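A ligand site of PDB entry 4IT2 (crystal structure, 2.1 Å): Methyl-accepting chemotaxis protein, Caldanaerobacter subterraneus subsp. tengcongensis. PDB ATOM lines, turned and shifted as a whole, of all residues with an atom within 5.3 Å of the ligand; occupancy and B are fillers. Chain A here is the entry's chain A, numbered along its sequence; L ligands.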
ATOM      1  N   MET A   1      22.765 -35.707  36.989  1.00  0.00           N
ATOM      2  CA  MET A   1      23.624 -34.550  36.734  1.00  0.00           C
ATOM      3  C   MET A   1      24.476 -34.264  37.970  1.00  0.00           C
ATOM      4  O   MET A   1      24.112 -34.673  39.078  1.00  0.00           O
ATOM      5  CB  MET A   1      22.774 -33.334  36.365  1.00  0.00           C
ATOM      6  CG  MET A   1      23.488 -32.290  35.491  1.00  0.00           C
ATOM      7  SD  MET A   1      23.755 -32.796  33.757  1.00  0.00           S
ATOM      8  CE  MET A   1      22.093 -33.323  33.335  1.00  0.00           C
ATOM      9  N   LYS A   2      25.593 -33.581  37.785  1.00  0.00           N
ATOM     10  CA  LYS A   2      26.440 -33.209  38.916  1.00  0.00           C
ATOM     11  C   LYS A   2      26.217 -31.773  39.295  1.00  0.00           C
ATOM     12  O   LYS A   2      25.841 -30.945  38.453  1.00  0.00           O
ATOM     13  CB  LYS A   2      27.918 -33.464  38.617  1.00  0.00           C
ATOM     14  CG  LYS A   2      28.258 -34.895  38.234  1.00  0.00           C
ATOM     15  CD  LYS A   2      27.545 -35.906  39.136  1.00  0.00           C
ATOM     16  CE  LYS A   2      28.031 -35.835  40.573  1.00  0.00           C
ATOM     17  NZ  LYS A   2      27.855 -37.151  41.258  1.00  0.00           N
ATOM     18  N   ILE A   5      27.329 -28.055  37.348  1.00  0.00           N
ATOM     19  CA  ILE A   5      26.568 -27.526  36.228  1.00  0.00           C
ATOM     20  C   ILE A   5      25.172 -27.132  36.694  1.00  0.00           C
ATOM     21  O   ILE A   5      24.691 -26.057  36.336  1.00  0.00           O
ATOM     22  CB  ILE A   5      26.535 -28.511  35.037  1.00  0.00           C
ATOM     23  CG1 ILE A   5      25.760 -27.914  33.853  1.00  0.00           C
ATOM     24  CG2 ILE A   5      25.954 -29.866  35.452  1.00  0.00           C
ATOM     25  CD1 ILE A   5      26.529 -26.855  33.089  1.00  0.00           C
ATOM     26  N   TRP A   9      23.217 -23.687  36.062  1.00  0.00           N
ATOM     27  CA  TRP A   9      21.863 -23.542  35.533  1.00  0.00           C
ATOM     28  C   TRP A   9      20.977 -22.693  36.442  1.00  0.00           C
ATOM     29  O   TRP A   9      20.214 -21.856  35.955  1.00  0.00           O
ATOM     30  CB  TRP A   9      21.235 -24.922  35.313  1.00  0.00           C
ATOM     31  CG  TRP A   9      21.904 -25.672  34.228  1.00  0.00           C
ATOM     32  CD1 TRP A   9      22.735 -25.154  33.275  1.00  0.00           C
ATOM     33  CD2 TRP A   9      21.824 -27.079  33.968  1.00  0.00           C
ATOM     34  NE1 TRP A   9      23.167 -26.148  32.441  1.00  0.00           N
ATOM     35  CE2 TRP A   9      22.625 -27.336  32.834  1.00  0.00           C
ATOM     36  CE3 TRP A   9      21.147 -28.149  34.566  1.00  0.00           C
ATOM     37  CZ2 TRP A   9      22.770 -28.614  32.306  1.00  0.00           C
ATOM     38  CZ3 TRP A   9      21.301 -29.417  34.040  1.00  0.00           C
ATOM     39  CH2 TRP A   9      22.102 -29.636  32.920  1.00  0.00           C
ATOM     40  N   ILE A  75      27.984 -20.185  27.759  1.00  0.00           N
ATOM     41  CA  ILE A  75      29.289 -20.049  27.108  1.00  0.00           C
ATOM     42  C   ILE A  75      30.086 -18.935  27.789  1.00  0.00           C
ATOM     43  O   ILE A  75      31.262 -19.094  28.107  1.00  0.00           O
ATOM     44  CB  ILE A  75      29.159 -19.764  25.593  1.00  0.00           C
ATOM     45  CG1 ILE A  75      28.531 -20.961  24.882  1.00  0.00           C
ATOM     46  CG2 ILE A  75      30.525 -19.445  24.991  1.00  0.00           C
ATOM     47  CD1 ILE A  75      29.347 -22.254  24.985  1.00  0.00           C
ATOM     48  N   PHE A  78      31.377 -20.218  31.042  1.00  0.00           N
ATOM     49  CA  PHE A  78      32.458 -21.165  30.797  1.00  0.00           C
ATOM     50  C   PHE A  78      33.756 -20.455  30.412  1.00  0.00           C
ATOM     51  O   PHE A  78      34.838 -20.887  30.807  1.00  0.00           O
ATOM     52  CB  PHE A  78      32.082 -22.182  29.724  1.00  0.00           C
ATOM     53  CG  PHE A  78      31.069 -23.199  30.166  1.00  0.00           C
ATOM     54  CD1 PHE A  78      30.832 -23.426  31.508  1.00  0.00           C
ATOM     55  CD2 PHE A  78      30.334 -23.921  29.222  1.00  0.00           C
ATOM     56  CE1 PHE A  78      29.888 -24.366  31.920  1.00  0.00           C
ATOM     57  CE2 PHE A  78      29.388 -24.856  29.620  1.00  0.00           C
ATOM     58  CZ  PHE A  78      29.170 -25.084  30.974  1.00  0.00           C
ATOM     59  N   PHE A  82      36.971 -21.251  32.590  1.00  0.00           N
ATOM     60  CA  PHE A  82      37.913 -22.102  31.877  1.00  0.00           C
ATOM     61  C   PHE A  82      38.434 -21.374  30.653  1.00  0.00           C
ATOM     62  O   PHE A  82      38.283 -21.853  29.548  1.00  0.00           O
ATOM     63  CB  PHE A  82      37.249 -23.431  31.468  1.00  0.00           C
ATOM     64  CG  PHE A  82      36.459 -24.070  32.574  1.00  0.00           C
ATOM     65  CD1 PHE A  82      37.086 -24.893  33.503  1.00  0.00           C
ATOM     66  CD2 PHE A  82      35.093 -23.836  32.708  1.00  0.00           C
ATOM     67  CE1 PHE A  82      36.365 -25.476  34.533  1.00  0.00           C
ATOM     68  CE2 PHE A  82      34.370 -24.414  33.725  1.00  0.00           C
ATOM     69  CZ  PHE A  82      35.008 -25.236  34.644  1.00  0.00           C
ATOM     70  N   TYR A  85      40.343 -22.846  27.496  1.00  0.00           N
ATOM     71  CA  TYR A  85      39.618 -23.512  26.417  1.00  0.00           C
ATOM     72  C   TYR A  85      39.266 -22.578  25.266  1.00  0.00           C
ATOM     73  O   TYR A  85      39.007 -23.005  24.139  1.00  0.00           O
ATOM     74  CB  TYR A  85      38.340 -24.125  26.979  1.00  0.00           C
ATOM     75  CG  TYR A  85      38.589 -25.389  27.752  1.00  0.00           C
ATOM     76  CD1 TYR A  85      37.841 -25.696  28.859  1.00  0.00           C
ATOM     77  CD2 TYR A  85      39.571 -26.279  27.354  1.00  0.00           C
ATOM     78  CE1 TYR A  85      38.070 -26.840  29.580  1.00  0.00           C
ATOM     79  CE2 TYR A  85      39.808 -27.438  28.061  1.00  0.00           C
ATOM     80  CZ  TYR A  85      39.042 -27.719  29.173  1.00  0.00           C
ATOM     81  OH  TYR A  85      39.266 -28.865  29.887  1.00  0.00           O
ATOM     82  N   PHE A  86      39.273 -21.286  25.558  1.00  0.00           N
ATOM     83  CA  PHE A  86      38.806 -20.284  24.598  1.00  0.00           C
ATOM     84  C   PHE A  86      39.950 -19.501  23.955  1.00  0.00           C
ATOM     85  O   PHE A  86      39.833 -19.056  22.802  1.00  0.00           O
ATOM     86  CB  PHE A  86      37.807 -19.339  25.287  1.00  0.00           C
ATOM     87  CG  PHE A  86      36.511 -20.025  25.688  1.00  0.00           C
ATOM     88  CD1 PHE A  86      35.348 -19.813  24.966  1.00  0.00           C
ATOM     89  CD2 PHE A  86      36.474 -20.889  26.774  1.00  0.00           C
ATOM     90  CE1 PHE A  86      34.159 -20.436  25.324  1.00  0.00           C
ATOM     91  CE2 PHE A  86      35.292 -21.518  27.129  1.00  0.00           C
ATOM     92  CZ  PHE A  86      34.139 -21.297  26.409  1.00  0.00           C
ATOM     93  N   PHE A  94      37.457 -24.793  18.606  1.00  0.00           N
ATOM     94  CA  PHE A  94      36.664 -24.984  19.817  1.00  0.00           C
ATOM     95  C   PHE A  94      35.651 -26.104  19.624  1.00  0.00           C
ATOM     96  O   PHE A  94      35.660 -27.099  20.356  1.00  0.00           O
ATOM     97  CB  PHE A  94      35.962 -23.678  20.165  1.00  0.00           C
ATOM     98  CG  PHE A  94      35.140 -23.737  21.423  1.00  0.00           C
ATOM     99  CD1 PHE A  94      35.757 -23.761  22.664  1.00  0.00           C
ATOM    100  CD2 PHE A  94      33.751 -23.766  21.356  1.00  0.00           C
ATOM    101  CE1 PHE A  94      34.999 -23.805  23.823  1.00  0.00           C
ATOM    102  CE2 PHE A  94      32.994 -23.819  22.505  1.00  0.00           C
ATOM    103  CZ  PHE A  94      33.611 -23.843  23.746  1.00  0.00           C
ATOM    104  N   LEU A  95      34.804 -25.973  18.617  1.00  0.00           N
ATOM    105  CA  LEU A  95      33.733 -26.949  18.396  1.00  0.00           C
ATOM    106  C   LEU A  95      34.283 -28.346  18.164  1.00  0.00           C
ATOM    107  O   LEU A  95      33.771 -29.329  18.704  1.00  0.00           O
ATOM    108  CB  LEU A  95      32.850 -26.508  17.220  1.00  0.00           C
ATOM    109  CG  LEU A  95      32.081 -25.217  17.467  1.00  0.00           C
ATOM    110  CD1 LEU A  95      31.298 -24.856  16.236  1.00  0.00           C
ATOM    111  CD2 LEU A  95      31.155 -25.336  18.683  1.00  0.00           C
ATOM    112  N   MET A  98      35.540 -30.099  21.365  1.00  0.00           N
ATOM    113  CA  MET A  98      34.560 -30.229  22.441  1.00  0.00           C
ATOM    114  C   MET A  98      34.336 -31.661  22.871  1.00  0.00           C
ATOM    115  O   MET A  98      34.159 -31.941  24.060  1.00  0.00           O
ATOM    116  CB  MET A  98      33.244 -29.554  22.063  1.00  0.00           C
ATOM    117  CG  MET A  98      33.238 -28.050  22.321  1.00  0.00           C
ATOM    118  SD  MET A  98      33.453 -27.670  24.089  1.00  0.00           S
ATOM    119  CE  MET A  98      35.159 -27.159  24.147  1.00  0.00           C
ATOM    120  N   VAL A 101      37.204 -32.670  25.284  1.00  0.00           N
ATOM    121  CA  VAL A 101      36.905 -32.034  26.558  1.00  0.00           C
ATOM    122  C   VAL A 101      35.989 -32.863  27.472  1.00  0.00           C
ATOM    123  O   VAL A 101      36.310 -33.100  28.627  1.00  0.00           O
ATOM    124  CB  VAL A 101      36.293 -30.639  26.335  1.00  0.00           C
ATOM    125  CG1 VAL A 101      35.797 -30.065  27.645  1.00  0.00           C
ATOM    126  CG2 VAL A 101      37.314 -29.703  25.687  1.00  0.00           C
ATOM    127  N   HIS A 102      34.862 -33.294  26.912  1.00  0.00           N
ATOM    128  CA  HIS A 102      33.855 -34.060  27.652  1.00  0.00           C
ATOM    129  C   HIS A 102      34.332 -35.439  28.089  1.00  0.00           C
ATOM    130  O   HIS A 102      34.014 -35.904  29.190  1.00  0.00           O
ATOM    131  CB  HIS A 102      32.590 -34.228  26.808  1.00  0.00           C
ATOM    132  CG  HIS A 102      31.731 -33.007  26.779  1.00  0.00           C
ATOM    133  ND1 HIS A 102      30.392 -33.036  26.444  1.00  0.00           N
ATOM    134  CD2 HIS A 102      32.020 -31.712  27.052  1.00  0.00           C
ATOM    135  CE1 HIS A 102      29.906 -31.815  26.523  1.00  0.00           C
ATOM    136  NE2 HIS A 102      30.865 -30.997  26.889  1.00  0.00           N
ATOM    137  N   LEU A 105      36.503 -34.915  30.796  1.00  0.00           N
ATOM    138  CA  LEU A 105      35.832 -34.249  31.912  1.00  0.00           C
ATOM    139  C   LEU A 105      35.133 -35.273  32.752  1.00  0.00           C
ATOM    140  O   LEU A 105      34.804 -35.021  33.914  1.00  0.00           O
ATOM    141  CB  LEU A 105      34.823 -33.214  31.413  1.00  0.00           C
ATOM    142  CG  LEU A 105      35.387 -31.801  31.366  1.00  0.00           C
ATOM    143  CD1 LEU A 105      34.262 -30.789  31.132  1.00  0.00           C
ATOM    144  CD2 LEU A 105      36.125 -31.511  32.655  1.00  0.00           C
ATOM    145  N   MET A 108      35.922 -35.414  36.274  1.00  0.00           N
ATOM    146  CA  MET A 108      35.537 -34.420  37.283  1.00  0.00           C
ATOM    147  C   MET A 108      34.883 -35.063  38.493  1.00  0.00           C
ATOM    148  O   MET A 108      35.355 -34.940  39.616  1.00  0.00           O
ATOM    149  CB  MET A 108      34.632 -33.331  36.694  1.00  0.00           C
ATOM    150  CG  MET A 108      35.408 -32.174  36.079  1.00  0.00           C
ATOM    151  SD  MET A 108      34.758 -30.522  36.454  1.00  0.00           S
ATOM    152  CE  MET A 108      36.061 -29.492  35.797  1.00  0.00           C
ATOM    153  N   ALA A 112      29.977 -38.618  36.344  1.00  0.00           N
ATOM    154  CA  ALA A 112      29.563 -37.674  35.307  1.00  0.00           C
ATOM    155  C   ALA A 112      29.360 -38.335  33.946  1.00  0.00           C
ATOM    156  O   ALA A 112      30.133 -39.195  33.535  1.00  0.00           O
ATOM    157  CB  ALA A 112      30.575 -36.526  35.197  1.00  0.00           C
ATOM    158  N   THR A 113      28.295 -37.931  33.239  1.00  0.00           N
ATOM    159  CA  THR A 113      28.061 -38.444  31.892  1.00  0.00           C
ATOM    160  C   THR A 113      27.685 -37.323  30.898  1.00  0.00           C
ATOM    161  O   THR A 113      26.541 -37.255  30.464  1.00  0.00           O
ATOM    162  CB  THR A 113      26.976 -39.542  31.858  1.00  0.00           C
ATOM    163  OG1 THR A 113      25.751 -39.043  32.415  1.00  0.00           O
ATOM    164  CG2 THR A 113      27.421 -40.773  32.646  1.00  0.00           C
ATOM    165  N   PRO A 114      28.643 -36.451  30.551  1.00  0.00           N
ATOM    166  CA  PRO A 114      28.350 -35.465  29.507  1.00  0.00           C
ATOM    167  C   PRO A 114      28.358 -36.166  28.146  1.00  0.00           C
ATOM    168  O   PRO A 114      29.046 -37.173  28.002  1.00  0.00           O
ATOM    169  CB  PRO A 114      29.506 -34.463  29.623  1.00  0.00           C
ATOM    170  CG  PRO A 114      30.635 -35.265  30.171  1.00  0.00           C
ATOM    171  CD  PRO A 114      30.020 -36.322  31.061  1.00  0.00           C
ATOM    172  N   PRO A 115      27.607 -35.642  27.168  1.00  0.00           N
ATOM    173  CA  PRO A 115      27.370 -36.349  25.903  1.00  0.00           C
ATOM    174  C   PRO A 115      28.573 -36.368  24.961  1.00  0.00           C
ATOM    175  O   PRO A 115      29.468 -35.537  25.068  1.00  0.00           O
ATOM    176  CB  PRO A 115      26.280 -35.503  25.241  1.00  0.00           C
ATOM    177  CG  PRO A 115      26.613 -34.113  25.686  1.00  0.00           C
ATOM    178  CD  PRO A 115      27.071 -34.268  27.129  1.00  0.00           C
ATOM    179  N   LEU A 117      30.164 -35.341  21.499  1.00  0.00           N
ATOM    180  CA  LEU A 117      29.980 -34.211  20.611  1.00  0.00           C
ATOM    181  C   LEU A 117      30.886 -34.333  19.386  1.00  0.00           C
ATOM    182  O   LEU A 117      31.531 -33.380  18.988  1.00  0.00           O
ATOM    183  CB  LEU A 117      30.312 -32.924  21.347  1.00  0.00           C
ATOM    184  CG  LEU A 117      29.439 -32.527  22.545  1.00  0.00           C
ATOM    185  CD1 LEU A 117      29.982 -31.234  23.146  1.00  0.00           C
ATOM    186  CD2 LEU A 117      27.970 -32.378  22.123  1.00  0.00           C
ATOM    187  N   MET A 129      28.195 -31.894  13.425  1.00  0.00           N
ATOM    188  CA  MET A 129      28.378 -32.230  14.820  1.00  0.00           C
ATOM    189  C   MET A 129      27.190 -33.056  15.287  1.00  0.00           C
ATOM    190  O   MET A 129      26.039 -32.739  14.961  1.00  0.00           O
ATOM    191  CB  MET A 129      28.521 -30.977  15.669  1.00  0.00           C
ATOM    192  CG  MET A 129      29.045 -31.270  17.064  1.00  0.00           C
ATOM    193  SD  MET A 129      29.091 -29.814  18.098  1.00  0.00           S
ATOM    194  CE  MET A 129      29.985 -28.686  17.062  1.00  0.00           C
ATOM    195  N   TYR A 131      25.369 -34.565  18.673  1.00  0.00           N
ATOM    196  CA  TYR A 131      25.099 -34.744  20.093  1.00  0.00           C
ATOM    197  C   TYR A 131      24.572 -36.158  20.323  1.00  0.00           C
ATOM    198  O   TYR A 131      23.649 -36.606  19.628  1.00  0.00           O
ATOM    199  CB  TYR A 131      24.072 -33.704  20.531  1.00  0.00           C
ATOM    200  CG  TYR A 131      23.350 -33.962  21.828  1.00  0.00           C
ATOM    201  CD1 TYR A 131      23.867 -33.486  23.034  1.00  0.00           C
ATOM    202  CD2 TYR A 131      22.128 -34.641  21.858  1.00  0.00           C
ATOM    203  CE1 TYR A 131      23.200 -33.687  24.226  1.00  0.00           C
ATOM    204  CE2 TYR A 131      21.451 -34.853  23.048  1.00  0.00           C
ATOM    205  CZ  TYR A 131      22.000 -34.365  24.238  1.00  0.00           C
ATOM    206  OH  TYR A 131      21.378 -34.554  25.441  1.00  0.00           O
ATOM    207  N   SER A 133      23.542 -38.694  23.662  1.00  0.00           N
ATOM    208  CA  SER A 133      23.386 -38.787  25.093  1.00  0.00           C
ATOM    209  C   SER A 133      22.221 -39.701  25.477  1.00  0.00           C
ATOM    210  O   SER A 133      21.379 -40.042  24.639  1.00  0.00           O
ATOM    211  CB  SER A 133      23.181 -37.389  25.684  1.00  0.00           C
ATOM    212  OG  SER A 133      22.861 -37.469  27.057  1.00  0.00           O
ATOM    213  N   ARG A 135      20.366 -38.486  27.620  1.00  0.00           N
ATOM    214  CA  ARG A 135      19.413 -37.423  27.855  1.00  0.00           C
ATOM    215  C   ARG A 135      18.969 -36.838  26.523  1.00  0.00           C
ATOM    216  O   ARG A 135      19.474 -37.225  25.464  1.00  0.00           O
ATOM    217  CB  ARG A 135      20.056 -36.340  28.713  1.00  0.00           C
ATOM    218  CG  ARG A 135      20.675 -36.887  29.981  1.00  0.00           C
ATOM    219  CD  ARG A 135      21.267 -35.777  30.804  1.00  0.00           C
ATOM    220  NE  ARG A 135      21.777 -36.284  32.070  1.00  0.00           N
ATOM    221  CZ  ARG A 135      23.051 -36.527  32.309  1.00  0.00           C
ATOM    222  NH1 ARG A 135      23.968 -36.289  31.368  1.00  0.00           N
ATOM    223  NH2 ARG A 135      23.426 -36.995  33.498  1.00  0.00           N
ATOM    224  N   MET A 137      18.705 -33.300  25.728  1.00  0.00           N
ATOM    225  CA  MET A 137      18.836 -31.862  25.975  1.00  0.00           C
ATOM    226  C   MET A 137      19.180 -31.112  24.677  1.00  0.00           C
ATOM    227  O   MET A 137      20.200 -30.418  24.566  1.00  0.00           O
ATOM    228  CB  MET A 137      19.833 -31.631  27.112  1.00  0.00           C
ATOM    229  CG  MET A 137      19.385 -32.350  28.379  1.00  0.00           C
ATOM    230  SD  MET A 137      20.522 -32.111  29.746  1.00  0.00           S
ATOM    231  CE  MET A 137      20.390 -30.342  29.910  1.00  0.00           C
ATOM    232  N   TYR A 140      19.425 -27.286  24.783  1.00  0.00           N
ATOM    233  CA  TYR A 140      20.589 -26.842  25.563  1.00  0.00           C
ATOM    234  C   TYR A 140      21.819 -26.915  24.657  1.00  0.00           C
ATOM    235  O   TYR A 140      22.567 -25.955  24.533  1.00  0.00           O
ATOM    236  CB  TYR A 140      20.757 -27.701  26.813  1.00  0.00           C
ATOM    237  CG  TYR A 140      21.917 -27.260  27.731  1.00  0.00           C
ATOM    238  CD1 TYR A 140      22.012 -25.967  28.191  1.00  0.00           C
ATOM    239  CD2 TYR A 140      22.868 -28.173  28.155  1.00  0.00           C
ATOM    240  CE1 TYR A 140      23.055 -25.564  29.031  1.00  0.00           C
ATOM    241  CE2 TYR A 140      23.921 -27.790  28.994  1.00  0.00           C
ATOM    242  CZ  TYR A 140      24.005 -26.490  29.420  1.00  0.00           C
ATOM    243  OH  TYR A 140      25.044 -26.104  30.255  1.00  0.00           O
ATOM    244  N   PHE A 141      21.964 -28.046  23.985  1.00  0.00           N
ATOM    245  CA  PHE A 141      22.970 -28.243  22.944  1.00  0.00           C
ATOM    246  C   PHE A 141      22.986 -27.129  21.884  1.00  0.00           C
ATOM    247  O   PHE A 141      24.018 -26.495  21.650  1.00  0.00           O
ATOM    248  CB  PHE A 141      22.741 -29.609  22.297  1.00  0.00           C
ATOM    249  CG  PHE A 141      23.595 -29.865  21.094  1.00  0.00           C
ATOM    250  CD1 PHE A 141      24.962 -30.068  21.216  1.00  0.00           C
ATOM    251  CD2 PHE A 141      23.012 -29.953  19.836  1.00  0.00           C
ATOM    252  CE1 PHE A 141      25.749 -30.333  20.098  1.00  0.00           C
ATOM    253  CE2 PHE A 141      23.784 -30.210  18.700  1.00  0.00           C
ATOM    254  CZ  PHE A 141      25.154 -30.397  18.828  1.00  0.00           C
ATOM    255  N   LEU A 144      24.071 -23.689  23.211  1.00  0.00           N
ATOM    256  CA  LEU A 144      25.513 -23.598  23.466  1.00  0.00           C
ATOM    257  C   LEU A 144      26.273 -23.326  22.161  1.00  0.00           C
ATOM    258  O   LEU A 144      27.198 -22.509  22.128  1.00  0.00           O
ATOM    259  CB  LEU A 144      26.011 -24.866  24.170  1.00  0.00           C
ATOM    260  CG  LEU A 144      25.653 -24.989  25.657  1.00  0.00           C
ATOM    261  CD1 LEU A 144      25.794 -26.420  26.120  1.00  0.00           C
ATOM    262  CD2 LEU A 144      26.501 -24.076  26.537  1.00  0.00           C
ATOM    263  N   ILE A 145      25.875 -23.997  21.083  1.00  0.00           N
ATOM    264  CA  ILE A 145      26.436 -23.714  19.764  1.00  0.00           C
ATOM    265  C   ILE A 145      26.261 -22.239  19.354  1.00  0.00           C
ATOM    266  O   ILE A 145      27.196 -21.599  18.864  1.00  0.00           O
ATOM    267  CB  ILE A 145      25.826 -24.638  18.692  1.00  0.00           C
ATOM    268  CG1 ILE A 145      26.446 -26.032  18.815  1.00  0.00           C
ATOM    269  CG2 ILE A 145      26.072 -24.087  17.300  1.00  0.00           C
ATOM    270  CD1 ILE A 145      25.784 -27.046  17.911  1.00  0.00           C
ATOM    271  N   SER A 148      28.438 -20.030  21.405  1.00  0.00           N
ATOM    272  CA  SER A 148      29.841 -20.141  21.013  1.00  0.00           C
ATOM    273  C   SER A 148      30.100 -19.235  19.810  1.00  0.00           C
ATOM    274  O   SER A 148      31.140 -18.592  19.715  1.00  0.00           O
ATOM    275  CB  SER A 148      30.199 -21.594  20.649  1.00  0.00           C
ATOM    276  OG  SER A 148      30.047 -22.468  21.753  1.00  0.00           O
HETATM  277 MN1  LIG L   1      29.264 -29.481  28.012  1.00  0.00          MN
HETATM  278  C1  LIG L   1      26.832 -31.096  30.116  1.00  0.00           C
HETATM  279  C2  LIG L   1      31.223 -29.082  30.696  1.00  0.00           C
HETATM  280  C3  LIG L   1      30.888 -26.745  26.459  1.00  0.00           C
HETATM  281  C4  LIG L   1      27.073 -29.548  25.500  1.00  0.00           C
HETATM  282  N1  LIG L   1      29.015 -29.937  30.044  1.00  0.00           N
HETATM  283  C5  LIG L   1      28.047 -30.720  30.663  1.00  0.00           C
HETATM  284  C6  LIG L   1      28.516 -31.066  31.988  1.00  0.00           C
HETATM  285  C7  LIG L   1      29.727 -30.500  32.139  1.00  0.00           C
HETATM  286  C8  LIG L   1      30.056 -29.785  30.929  1.00  0.00           C
HETATM  287  C9  LIG L   1      30.618 -30.604  33.408  1.00  0.00           C
HETATM  288  C10 LIG L   1      27.772 -31.913  33.047  1.00  0.00           C
HETATM  289  C11 LIG L   1      28.022 -33.398  32.836  1.00  0.00           C
HETATM  290  C12 LIG L   1      27.271 -34.232  33.856  1.00  0.00           C
HETATM  291  O1  LIG L   1      27.025 -35.441  33.599  1.00  0.00           O
HETATM  292  O2  LIG L   1      26.900 -33.687  34.927  1.00  0.00           O
HETATM  293  N2  LIG L   1      30.729 -28.128  28.477  1.00  0.00           N
HETATM  294  C13 LIG L   1      31.465 -28.217  29.642  1.00  0.00           C
HETATM  295  C14 LIG L   1      32.552 -27.248  29.597  1.00  0.00           C
HETATM  296  C15 LIG L   1      32.455 -26.604  28.415  1.00  0.00           C
HETATM  297  C16 LIG L   1      31.312 -27.143  27.704  1.00  0.00           C
HETATM  298  C17 LIG L   1      33.582 -27.060  30.735  1.00  0.00           C
HETATM  299  C18 LIG L   1      33.333 -25.473  27.819  1.00  0.00           C
HETATM  300  C19 LIG L   1      34.388 -24.932  28.440  1.00  0.00           C
HETATM  301  N3  LIG L   1      29.014 -28.291  26.356  1.00  0.00           N
HETATM  302  C20 LIG L   1      29.847 -27.346  25.805  1.00  0.00           C
HETATM  303  C21 LIG L   1      29.445 -27.109  24.437  1.00  0.00           C
HETATM  304  C22 LIG L   1      28.381 -27.883  24.182  1.00  0.00           C
HETATM  305  C23 LIG L   1      28.095 -28.641  25.383  1.00  0.00           C
HETATM  306  C24 LIG L   1      30.132 -26.112  23.481  1.00  0.00           C
HETATM  307  C25 LIG L   1      27.561 -28.048  22.878  1.00  0.00           C
HETATM  308  C26 LIG L   1      28.053 -27.757  21.666  1.00  0.00           C
HETATM  309  N4  LIG L   1      27.245 -30.242  27.842  1.00  0.00           N
HETATM  310  C27 LIG L   1      26.555 -30.073  26.653  1.00  0.00           C
HETATM  311  C28 LIG L   1      25.197 -30.551  26.820  1.00  0.00           C
HETATM  312  C29 LIG L   1      25.121 -31.041  28.266  1.00  0.00           C
HETATM  313  C30 LIG L   1      26.431 -30.803  28.821  1.00  0.00           C
HETATM  314  C31 LIG L   1      24.064 -30.572  25.778  1.00  0.00           C
HETATM  315  C32 LIG L   1      23.884 -31.638  28.964  1.00  0.00           C
HETATM  316  C33 LIG L   1      24.104 -33.093  29.343  1.00  0.00           C
HETATM  317  C34 LIG L   1      23.526 -33.992  28.289  1.00  0.00           C
HETATM  318  O3  LIG L   1      22.982 -33.477  27.278  1.00  0.00           O
HETATM  319  O4  LIG L   1      23.579 -35.239  28.454  1.00  0.00           O
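A ring nitrogen (NE2) of His 102 is bound to a manganese atom (MN1) of the ligand (2.5 Å). The side-chain hydroxyl of Ser 133 sits at hydrogen-bond distance from an oxygen (O4) of the ligand (2.7 Å). An oxygen (O4) of the ligand is in salt-bridge range of the guanidinium group (NH1) of Arg 135 (3.1 Å). O3 of the ligand is in hydrogen-bond range of OH of Tyr 131 (2.7 Å). N of Lys 2 sits at hydrogen-bond distance from O2 of the ligand (3.1 Å). The backbone NH (N) of Thr 113 is in hydrogen-bond range of an oxygen (O1) of the ligand, 2.8 Å away.
The side-chain hydroxyl (OG) of Ser 148 lies within hydrogen-bond range of the backbone carbonyl oxygen (O) of Leu 144 (2.9 Å). OH of Tyr 131 sits at hydrogen-bond distance from O of Arg 135 (3.3 Å). O of Thr 113 sits at hydrogen-bond distance from NH1 of Arg 135, at 2.9 Å. ND1 of His 102 is in hydrogen-bond range of O of Pro 115. The side-chain hydroxyl (OH) of Tyr 131 sits at hydrogen-bond distance from the backbone NH (N) of Met 137, at 3.0 Å. OG of Ser 133 is in hydrogen-bond range of N of Arg 135, 2.8 Å away. OH of Tyr 140 sits at hydrogen-bond distance from NE1 of Trp 9 (2.9 Å).
An oxygen (O2) of the ligand sits close to the side-chain sulfur (SD) of Met 1. The side-chain sulfur of Met 137 lies close to an oxygen (O3) of the ligand, at 3.7 Å. CG2 of Ile 5 touches C10 of the ligand, 3.6 Å away. Phe 78 touches the ligand. Tyr 85 touches the ligand. CE2 of Phe 86 touches C19 of the ligand, at 3.8 Å. CE2 of Phe 94 touches C24 of the ligand (3.8 Å). Met 98 touches the ligand (SD to C3, 3.6 Å). Leu 105 touches the ligand. C of Ala 112 touches O1 of the ligand, 3.7 Å away. N of Pro 114 touches O1 of the ligand (3.6 Å). Pro 115 touches the ligand (CD to C34, 3.7 Å). Leu 117 touches the ligand. Tyr 140 touches the ligand. Phe 141 touches the ligand. CD1 of Leu 144 touches C23 of the ligand, at 3.3 Å. CG1 of Ile 145 touches C26 of the ligand, 3.7 Å away. Within 4 Å of the ligand: Met 1, Lys 2, Ile 5, Phe 78, Tyr 85, Phe 86, Phe 94, Met 98, His 102, Leu 105, Ala 112, Thr 113, Pro 114, Pro 115, Leu 117, Tyr 131, Ser 133, Arg 135, Met 137, Tyr 140, Phe 141, Leu 144 and Ile 145.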
